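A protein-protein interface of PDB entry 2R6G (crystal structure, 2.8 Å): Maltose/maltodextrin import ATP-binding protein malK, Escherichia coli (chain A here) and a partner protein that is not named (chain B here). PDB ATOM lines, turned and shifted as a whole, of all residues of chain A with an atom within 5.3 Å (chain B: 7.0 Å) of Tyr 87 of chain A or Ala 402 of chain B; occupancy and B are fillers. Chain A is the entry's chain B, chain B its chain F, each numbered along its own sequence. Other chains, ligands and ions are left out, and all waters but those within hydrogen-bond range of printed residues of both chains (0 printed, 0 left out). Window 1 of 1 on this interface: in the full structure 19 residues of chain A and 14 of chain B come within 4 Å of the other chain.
Of the 15 printed residues of chain B, 9 touch a printed residue of chain A.
Printed residues of chain B that touch a printed residue of chain A: Asp 398, Leu 399, Glu 401, Ala 402, Ser 403, Met 405, Asp 406, Lys 416 and Ile 417.
Hydrophobic or aromatic side chains of chain B that line the printed part of chain A: Leu 399, Ala 402, Met 405 and Ile 417.
Of the 12 printed residues of chain A, 8 touch a printed residue of chain B.
Among the printed residues, 17 pairs touch across the chains.
Of the printed residues of chain B, Ala 85 of chain A touches Asp 398, Leu 399 and Ala 402.
Printed residues of chain B within 4 Å of Pro 88 of chain A: Leu 399 (3.7 Å).
Of the printed residues of chain B, Arg 146 of chain A touches Ala 402 and Asp 406.
Ala 402 of chain B touches just these residues of chain A: Phe 81 (3.9 Å), Ala 85 (3.6 Å), Tyr 87 (2.9 Å) and Arg 146 (3.4 Å).
Of the printed residues of chain A, Lys 416 of chain B touches His 89.
The nearest residue of chain B that does not touch Tyr 87 of chain A is Ala 404 of chain B (5.6 Å).
The nearest printed residue of chain A that does not touch Ala 402 of chain B is Phe 98 of chain A (5.4 Å).
The nearest printed residue of chain A that does not touch Asp 406 of chain B is Asn 95 of chain A (4.6 Å).
The backbone carbonyl oxygen (O) of Ser 403 of chain B sits at hydrogen-bond distance from the backbone NH (N) of Ala 408 of chain B (3.1 Å).
The backbone carbonyl oxygen (O) of Ala 85 of chain A lies within hydrogen-bond range of the guanidinium group (NH2) of Arg 146 of chain A (2.7 Å).
The backbone NH (N) of Tyr 87 of chain A sits at hydrogen-bond distance from the side-chain amide oxygen (OD1) of Asn 95 of chain A, at 2.8 Å.
The backbone carbonyl oxygen of Leu 399 of chain B lies within hydrogen-bond range of the side-chain hydroxyl of Ser 403 of chain B, 2.9 Å away.
O of Glu 401 of chain B touches CZ of Phe 81 of chain A, at 3.6 Å.
Ala 402 of chain B touches Phe 81 of chain A (CA to CE1, 3.9 Å).
Met 405 of chain B touches Phe 81 of chain A.
Leu 399 of chain B touches Ala 85 of chain A (CD2 to O, 3.8 Å).
O of Ala 85 of chain A touches CB of Ala 402 of chain B, at 3.6 Å.
CD2 of Leu 399 of chain B touches O of Leu 86 of chain A (3.3 Å).
Asp 406 of chain B touches Tyr 87 of chain A.
Tyr 87 of chain A touches Ile 417 of chain B.
Pro 88 of chain A touches Leu 399 of chain B.
Arg 146 of chain A touches Asp 406 of chain B.
The side-chain hydroxyl (OH) of Tyr 87 of chain A lies within hydrogen-bond range of the backbone NH (N) of Ser 403 of chain B (3.4 Å).
NE2 of His 89 of chain A lies within hydrogen-bond range of O of Lys 416 of chain B, at 3.3 Å.
The side-chain hydroxyl (OH) of Tyr 87 of chain A is in hydrogen-bond range of the backbone carbonyl oxygen (O) of Ala 402 of chain B (2.9 Å).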
ATOM      1  N   PHE A  81      -0.328 -29.943 -13.221  1.00  0.00           N
ATOM      2  CA  PHE A  81      -1.371 -30.125 -14.234  1.00  0.00           C
ATOM      3  C   PHE A  81      -0.892 -29.923 -15.671  1.00  0.00           C
ATOM      4  O   PHE A  81       0.119 -29.258 -15.904  1.00  0.00           O
ATOM      5  CB  PHE A  81      -2.554 -29.193 -13.933  1.00  0.00           C
ATOM      6  CG  PHE A  81      -3.275 -29.524 -12.654  1.00  0.00           C
ATOM      7  CD1 PHE A  81      -2.812 -29.040 -11.429  1.00  0.00           C
ATOM      8  CD2 PHE A  81      -4.414 -30.324 -12.672  1.00  0.00           C
ATOM      9  CE1 PHE A  81      -3.473 -29.349 -10.243  1.00  0.00           C
ATOM     10  CE2 PHE A  81      -5.084 -30.637 -11.494  1.00  0.00           C
ATOM     11  CZ  PHE A  81      -4.613 -30.149 -10.276  1.00  0.00           C
ATOM     12  N   ALA A  85      -3.270 -24.401 -13.754  1.00  0.00           N
ATOM     13  CA  ALA A  85      -4.157 -24.188 -12.613  1.00  0.00           C
ATOM     14  C   ALA A  85      -3.503 -23.358 -11.512  1.00  0.00           C
ATOM     15  O   ALA A  85      -3.719 -23.601 -10.325  1.00  0.00           O
ATOM     16  CB  ALA A  85      -4.665 -25.528 -12.066  1.00  0.00           C
ATOM     17  N   LEU A  86      -2.703 -22.375 -11.917  1.00  0.00           N
ATOM     18  CA  LEU A  86      -2.034 -21.494 -10.968  1.00  0.00           C
ATOM     19  C   LEU A  86      -3.059 -20.615 -10.265  1.00  0.00           C
ATOM     20  O   LEU A  86      -4.070 -20.240 -10.860  1.00  0.00           O
ATOM     21  CB  LEU A  86      -0.975 -20.632 -11.664  1.00  0.00           C
ATOM     22  CG  LEU A  86       0.088 -21.285 -12.561  1.00  0.00           C
ATOM     23  CD1 LEU A  86       1.204 -20.285 -12.845  1.00  0.00           C
ATOM     24  CD2 LEU A  86       0.672 -22.561 -11.964  1.00  0.00           C
ATOM     25  N   TYR A  87      -2.811 -20.309  -8.995  1.00  0.00           N
ATOM     26  CA  TYR A  87      -3.693 -19.425  -8.248  1.00  0.00           C
ATOM     27  C   TYR A  87      -3.463 -17.998  -8.738  1.00  0.00           C
ATOM     28  O   TYR A  87      -2.370 -17.456  -8.554  1.00  0.00           O
ATOM     29  CB  TYR A  87      -3.450 -19.546  -6.739  1.00  0.00           C
ATOM     30  CG  TYR A  87      -3.480 -20.968  -6.212  1.00  0.00           C
ATOM     31  CD1 TYR A  87      -2.324 -21.569  -5.726  1.00  0.00           C
ATOM     32  CD2 TYR A  87      -4.661 -21.708  -6.201  1.00  0.00           C
ATOM     33  CE1 TYR A  87      -2.338 -22.870  -5.244  1.00  0.00           C
ATOM     34  CE2 TYR A  87      -4.687 -23.015  -5.716  1.00  0.00           C
ATOM     35  CZ  TYR A  87      -3.521 -23.586  -5.239  1.00  0.00           C
ATOM     36  OH  TYR A  87      -3.527 -24.875  -4.757  1.00  0.00           O
ATOM     37  N   PRO A  88      -4.489 -17.390  -9.370  1.00  0.00           N
ATOM     38  CA  PRO A  88      -4.331 -16.107 -10.065  1.00  0.00           C
ATOM     39  C   PRO A  88      -4.159 -14.926  -9.113  1.00  0.00           C
ATOM     40  O   PRO A  88      -3.529 -13.931  -9.469  1.00  0.00           O
ATOM     41  CB  PRO A  88      -5.640 -15.973 -10.845  1.00  0.00           C
ATOM     42  CG  PRO A  88      -6.630 -16.729 -10.040  1.00  0.00           C
ATOM     43  CD  PRO A  88      -5.880 -17.880  -9.439  1.00  0.00           C
ATOM     44  N   HIS A  89      -4.709 -15.055  -7.910  1.00  0.00           N
ATOM     45  CA  HIS A  89      -4.688 -13.993  -6.912  1.00  0.00           C
ATOM     46  C   HIS A  89      -3.403 -13.983  -6.086  1.00  0.00           C
ATOM     47  O   HIS A  89      -3.178 -13.070  -5.290  1.00  0.00           O
ATOM     48  CB  HIS A  89      -5.911 -14.115  -5.994  1.00  0.00           C
ATOM     49  CG  HIS A  89      -6.065 -15.464  -5.358  1.00  0.00           C
ATOM     50  ND1 HIS A  89      -6.273 -16.613  -6.090  1.00  0.00           N
ATOM     51  CD2 HIS A  89      -6.059 -15.841  -4.059  1.00  0.00           C
ATOM     52  CE1 HIS A  89      -6.378 -17.643  -5.268  1.00  0.00           C
ATOM     53  NE2 HIS A  89      -6.253 -17.202  -4.030  1.00  0.00           N
ATOM     54  N   LEU A  90      -2.564 -14.996  -6.287  1.00  0.00           N
ATOM     55  CA  LEU A  90      -1.331 -15.143  -5.520  1.00  0.00           C
ATOM     56  C   LEU A  90      -0.095 -15.094  -6.408  1.00  0.00           C
ATOM     57  O   LEU A  90      -0.120 -15.562  -7.547  1.00  0.00           O
ATOM     58  CB  LEU A  90      -1.353 -16.450  -4.723  1.00  0.00           C
ATOM     59  CG  LEU A  90      -2.429 -16.576  -3.642  1.00  0.00           C
ATOM     60  CD1 LEU A  90      -2.656 -18.033  -3.291  1.00  0.00           C
ATOM     61  CD2 LEU A  90      -2.062 -15.767  -2.407  1.00  0.00           C
ATOM     62  N   SER A  91       0.985 -14.531  -5.871  1.00  0.00           N
ATOM     63  CA  SER A  91       2.255 -14.412  -6.583  1.00  0.00           C
ATOM     64  C   SER A  91       2.921 -15.773  -6.774  1.00  0.00           C
ATOM     65  O   SER A  91       2.420 -16.788  -6.289  1.00  0.00           O
ATOM     66  CB  SER A  91       3.198 -13.474  -5.824  1.00  0.00           C
ATOM     67  OG  SER A  91       3.621 -14.057  -4.603  1.00  0.00           O
ATOM     68  N   ASN A  95       2.248 -18.966  -4.602  1.00  0.00           N
ATOM     69  CA  ASN A  95       1.820 -20.173  -5.313  1.00  0.00           C
ATOM     70  C   ASN A  95       2.630 -21.393  -4.891  1.00  0.00           C
ATOM     71  O   ASN A  95       2.068 -22.428  -4.533  1.00  0.00           O
ATOM     72  CB  ASN A  95       1.932 -19.981  -6.829  1.00  0.00           C
ATOM     73  CG  ASN A  95       0.636 -19.514  -7.460  1.00  0.00           C
ATOM     74  OD1 ASN A  95      -0.263 -20.312  -7.722  1.00  0.00           O
ATOM     75  ND2 ASN A  95       0.542 -18.219  -7.732  1.00  0.00           N
ATOM     76  N   PHE A  98       2.444 -22.916  -0.838  1.00  0.00           N
ATOM     77  CA  PHE A  98       1.017 -23.054  -0.571  1.00  0.00           C
ATOM     78  C   PHE A  98       0.687 -24.411   0.031  1.00  0.00           C
ATOM     79  O   PHE A  98      -0.115 -24.497   0.959  1.00  0.00           O
ATOM     80  CB  PHE A  98       0.204 -22.826  -1.847  1.00  0.00           C
ATOM     81  CG  PHE A  98      -1.272 -22.684  -1.609  1.00  0.00           C
ATOM     82  CD1 PHE A  98      -1.797 -21.501  -1.095  1.00  0.00           C
ATOM     83  CD2 PHE A  98      -2.141 -23.731  -1.904  1.00  0.00           C
ATOM     84  CE1 PHE A  98      -3.163 -21.364  -0.876  1.00  0.00           C
ATOM     85  CE2 PHE A  98      -3.509 -23.602  -1.693  1.00  0.00           C
ATOM     86  CZ  PHE A  98      -4.021 -22.417  -1.177  1.00  0.00           C
ATOM     87  N   PRO A 131       0.702 -14.558 -11.752  1.00  0.00           N
ATOM     88  CA  PRO A 131       0.738 -15.507 -12.878  1.00  0.00           C
ATOM     89  C   PRO A 131       0.472 -14.914 -14.261  1.00  0.00           C
ATOM     90  O   PRO A 131       1.175 -15.259 -15.209  1.00  0.00           O
ATOM     91  CB  PRO A 131      -0.353 -16.524 -12.522  1.00  0.00           C
ATOM     92  CG  PRO A 131      -0.463 -16.445 -11.049  1.00  0.00           C
ATOM     93  CD  PRO A 131      -0.255 -14.995 -10.720  1.00  0.00           C
ATOM     94  N   ARG A 146       5.303 -25.714  -7.311  1.00  0.00           N
ATOM     95  CA  ARG A 146       4.255 -25.894  -6.309  1.00  0.00           C
ATOM     96  C   ARG A 146       4.211 -27.326  -5.761  1.00  0.00           C
ATOM     97  O   ARG A 146       4.001 -27.533  -4.564  1.00  0.00           O
ATOM     98  CB  ARG A 146       2.896 -25.518  -6.904  1.00  0.00           C
ATOM     99  CG  ARG A 146       1.812 -25.255  -5.876  1.00  0.00           C
ATOM    100  CD  ARG A 146       0.448 -25.613  -6.428  1.00  0.00           C
ATOM    101  NE  ARG A 146      -0.067 -24.619  -7.364  1.00  0.00           N
ATOM    102  CZ  ARG A 146      -0.924 -24.884  -8.346  1.00  0.00           C
ATOM    103  NH1 ARG A 146      -1.364 -26.119  -8.552  1.00  0.00           N
ATOM    104  NH2 ARG A 146      -1.334 -23.911  -9.137  1.00  0.00           N
ATOM    105  N   ASP B 397     -13.257 -24.460 -11.541  1.00  0.00           N
ATOM    106  CA  ASP B 397     -13.165 -25.688 -10.739  1.00  0.00           C
ATOM    107  C   ASP B 397     -11.740 -26.199 -10.535  1.00  0.00           C
ATOM    108  O   ASP B 397     -11.415 -26.716  -9.466  1.00  0.00           O
ATOM    109  CB  ASP B 397     -14.013 -26.802 -11.362  1.00  0.00           C
ATOM    110  CG  ASP B 397     -15.437 -26.369 -11.644  1.00  0.00           C
ATOM    111  OD1 ASP B 397     -15.737 -26.092 -12.823  1.00  0.00           O
ATOM    112  OD2 ASP B 397     -16.250 -26.294 -10.698  1.00  0.00           O
ATOM    113  N   ASP B 398     -10.900 -26.059 -11.560  1.00  0.00           N
ATOM    114  CA  ASP B 398      -9.515 -26.550 -11.511  1.00  0.00           C
ATOM    115  C   ASP B 398      -8.660 -25.881 -10.425  1.00  0.00           C
ATOM    116  O   ASP B 398      -7.620 -26.417 -10.032  1.00  0.00           O
ATOM    117  CB  ASP B 398      -8.838 -26.477 -12.890  1.00  0.00           C
ATOM    118  CG  ASP B 398      -8.819 -25.072 -13.473  1.00  0.00           C
ATOM    119  OD1 ASP B 398      -9.638 -24.222 -13.063  1.00  0.00           O
ATOM    120  OD2 ASP B 398      -7.978 -24.820 -14.361  1.00  0.00           O
ATOM    121  N   LEU B 399      -9.100 -24.720  -9.942  1.00  0.00           N
ATOM    122  CA  LEU B 399      -8.444 -24.061  -8.813  1.00  0.00           C
ATOM    123  C   LEU B 399      -8.644 -24.836  -7.510  1.00  0.00           C
ATOM    124  O   LEU B 399      -7.767 -24.846  -6.644  1.00  0.00           O
ATOM    125  CB  LEU B 399      -8.921 -22.614  -8.665  1.00  0.00           C
ATOM    126  CG  LEU B 399      -8.248 -21.579  -9.570  1.00  0.00           C
ATOM    127  CD1 LEU B 399      -8.883 -20.216  -9.386  1.00  0.00           C
ATOM    128  CD2 LEU B 399      -6.751 -21.502  -9.304  1.00  0.00           C
ATOM    129  N   TYR B 400      -9.801 -25.481  -7.387  1.00  0.00           N
ATOM    130  CA  TYR B 400     -10.098 -26.343  -6.249  1.00  0.00           C
ATOM    131  C   TYR B 400      -9.445 -27.706  -6.420  1.00  0.00           C
ATOM    132  O   TYR B 400      -9.196 -28.411  -5.439  1.00  0.00           O
ATOM    133  CB  TYR B 400     -11.609 -26.488  -6.058  1.00  0.00           C
ATOM    134  CG  TYR B 400     -12.294 -25.205  -5.649  1.00  0.00           C
ATOM    135  CD1 TYR B 400     -13.114 -24.515  -6.540  1.00  0.00           C
ATOM    136  CD2 TYR B 400     -12.112 -24.671  -4.372  1.00  0.00           C
ATOM    137  CE1 TYR B 400     -13.741 -23.330  -6.166  1.00  0.00           C
ATOM    138  CE2 TYR B 400     -12.732 -23.490  -3.989  1.00  0.00           C
ATOM    139  CZ  TYR B 400     -13.546 -22.826  -4.888  1.00  0.00           C
ATOM    140  OH  TYR B 400     -14.160 -21.658  -4.509  1.00  0.00           O
ATOM    141  N   GLU B 401      -9.175 -28.071  -7.674  1.00  0.00           N
ATOM    142  CA  GLU B 401      -8.403 -29.271  -7.984  1.00  0.00           C
ATOM    143  C   GLU B 401      -6.945 -29.058  -7.596  1.00  0.00           C
ATOM    144  O   GLU B 401      -6.277 -29.985  -7.144  1.00  0.00           O
ATOM    145  CB  GLU B 401      -8.509 -29.626  -9.468  1.00  0.00           C
ATOM    146  CG  GLU B 401      -9.906 -30.032  -9.913  1.00  0.00           C
ATOM    147  CD  GLU B 401      -9.921 -30.720 -11.264  1.00  0.00           C
ATOM    148  OE1 GLU B 401      -9.337 -30.178 -12.227  1.00  0.00           O
ATOM    149  OE2 GLU B 401     -10.524 -31.808 -11.364  1.00  0.00           O
ATOM    150  N   ALA B 402      -6.468 -27.826  -7.774  1.00  0.00           N
ATOM    151  CA  ALA B 402      -5.133 -27.429  -7.338  1.00  0.00           C
ATOM    152  C   ALA B 402      -5.063 -27.361  -5.819  1.00  0.00           C
ATOM    153  O   ALA B 402      -4.029 -27.667  -5.230  1.00  0.00           O
ATOM    154  CB  ALA B 402      -4.750 -26.092  -7.944  1.00  0.00           C
ATOM    155  N   SER B 403      -6.167 -26.952  -5.196  1.00  0.00           N
ATOM    156  CA  SER B 403      -6.280 -26.914  -3.739  1.00  0.00           C
ATOM    157  C   SER B 403      -6.111 -28.309  -3.145  1.00  0.00           C
ATOM    158  O   SER B 403      -5.365 -28.499  -2.180  1.00  0.00           O
ATOM    159  CB  SER B 403      -7.639 -26.352  -3.321  1.00  0.00           C
ATOM    160  OG  SER B 403      -7.813 -25.025  -3.774  1.00  0.00           O
ATOM    161  N   ALA B 404      -6.809 -29.273  -3.741  1.00  0.00           N
ATOM    162  CA  ALA B 404      -6.799 -30.656  -3.282  1.00  0.00           C
ATOM    163  C   ALA B 404      -5.402 -31.259  -3.344  1.00  0.00           C
ATOM    164  O   ALA B 404      -4.980 -31.953  -2.419  1.00  0.00           O
ATOM    165  CB  ALA B 404      -7.775 -31.485  -4.098  1.00  0.00           C
ATOM    166  N   MET B 405      -4.684 -30.975  -4.430  1.00  0.00           N
ATOM    167  CA  MET B 405      -3.339 -31.512  -4.628  1.00  0.00           C
ATOM    168  C   MET B 405      -2.307 -30.887  -3.688  1.00  0.00           C
ATOM    169  O   MET B 405      -1.243 -31.462  -3.464  1.00  0.00           O
ATOM    170  CB  MET B 405      -2.910 -31.396  -6.094  1.00  0.00           C
ATOM    171  CG  MET B 405      -3.820 -32.138  -7.072  1.00  0.00           C
ATOM    172  SD  MET B 405      -4.408 -33.746  -6.490  1.00  0.00           S
ATOM    173  CE  MET B 405      -2.940 -34.743  -6.672  1.00  0.00           C
ATOM    174  N   ASP B 406      -2.628 -29.713  -3.147  1.00  0.00           N
ATOM    175  CA  ASP B 406      -1.825 -29.098  -2.092  1.00  0.00           C
ATOM    176  C   ASP B 406      -2.326 -29.529  -0.712  1.00  0.00           C
ATOM    177  O   ASP B 406      -1.741 -29.167   0.313  1.00  0.00           O
ATOM    178  CB  ASP B 406      -1.840 -27.571  -2.217  1.00  0.00           C
ATOM    179  CG  ASP B 406      -0.980 -27.066  -3.367  1.00  0.00           C
ATOM    180  OD1 ASP B 406      -1.157 -27.539  -4.511  1.00  0.00           O
ATOM    181  OD2 ASP B 406      -0.132 -26.180  -3.123  1.00  0.00           O
ATOM    182  N   GLY B 407      -3.409 -30.303  -0.697  1.00  0.00           N
ATOM    183  CA  GLY B 407      -3.987 -30.827   0.538  1.00  0.00           C
ATOM    184  C   GLY B 407      -4.807 -29.792   1.278  1.00  0.00           C
ATOM    185  O   GLY B 407      -4.385 -29.288   2.320  1.00  0.00           O
ATOM    186  N   ALA B 408      -5.985 -29.480   0.743  1.00  0.00           N
ATOM    187  CA  ALA B 408      -6.842 -28.443   1.315  1.00  0.00           C
ATOM    188  C   ALA B 408      -8.331 -28.773   1.241  1.00  0.00           C
ATOM    189  O   ALA B 408      -8.749 -29.642   0.471  1.00  0.00           O
ATOM    190  CB  ALA B 408      -6.567 -27.110   0.637  1.00  0.00           C
ATOM    191  N   ASN B 413     -10.059 -24.398   1.874  1.00  0.00           N
ATOM    192  CA  ASN B 413     -10.531 -23.872   0.593  1.00  0.00           C
ATOM    193  C   ASN B 413     -11.238 -22.535   0.744  1.00  0.00           C
ATOM    194  O   ASN B 413     -10.976 -21.603  -0.011  1.00  0.00           O
ATOM    195  CB  ASN B 413     -11.476 -24.867  -0.088  1.00  0.00           C
ATOM    196  CG  ASN B 413     -10.745 -25.898  -0.922  1.00  0.00           C
ATOM    197  OD1 ASN B 413     -11.333 -26.522  -1.803  1.00  0.00           O
ATOM    198  ND2 ASN B 413      -9.459 -26.083  -0.651  1.00  0.00           N
ATOM    199  N   LYS B 416      -8.770 -19.563   1.906  1.00  0.00           N
ATOM    200  CA  LYS B 416      -7.588 -19.372   1.061  1.00  0.00           C
ATOM    201  C   LYS B 416      -7.908 -19.217  -0.429  1.00  0.00           C
ATOM    202  O   LYS B 416      -7.096 -18.674  -1.180  1.00  0.00           O
ATOM    203  CB  LYS B 416      -6.559 -20.491   1.281  1.00  0.00           C
ATOM    204  CG  LYS B 416      -6.162 -20.736   2.748  1.00  0.00           C
ATOM    205  CD  LYS B 416      -5.600 -19.492   3.441  1.00  0.00           C
ATOM    206  CE  LYS B 416      -4.140 -19.255   3.089  1.00  0.00           C
ATOM    207  NZ  LYS B 416      -3.628 -17.986   3.677  1.00  0.00           N
ATOM    208  N   ILE B 417      -9.086 -19.683  -0.849  1.00  0.00           N
ATOM    209  CA  ILE B 417      -9.515 -19.569  -2.252  1.00  0.00           C
ATOM    210  C   ILE B 417     -10.817 -18.776  -2.403  1.00  0.00           C
ATOM    211  O   ILE B 417     -10.791 -17.625  -2.834  1.00  0.00           O
ATOM    212  CB  ILE B 417      -9.648 -20.961  -2.957  1.00  0.00           C
ATOM    213  CG1 ILE B 417      -8.355 -21.789  -2.837  1.00  0.00           C
ATOM    214  CG2 ILE B 417     -10.087 -20.804  -4.420  1.00  0.00           C
ATOM    215  CD1 ILE B 417      -7.134 -21.209  -3.538  1.00  0.00           C
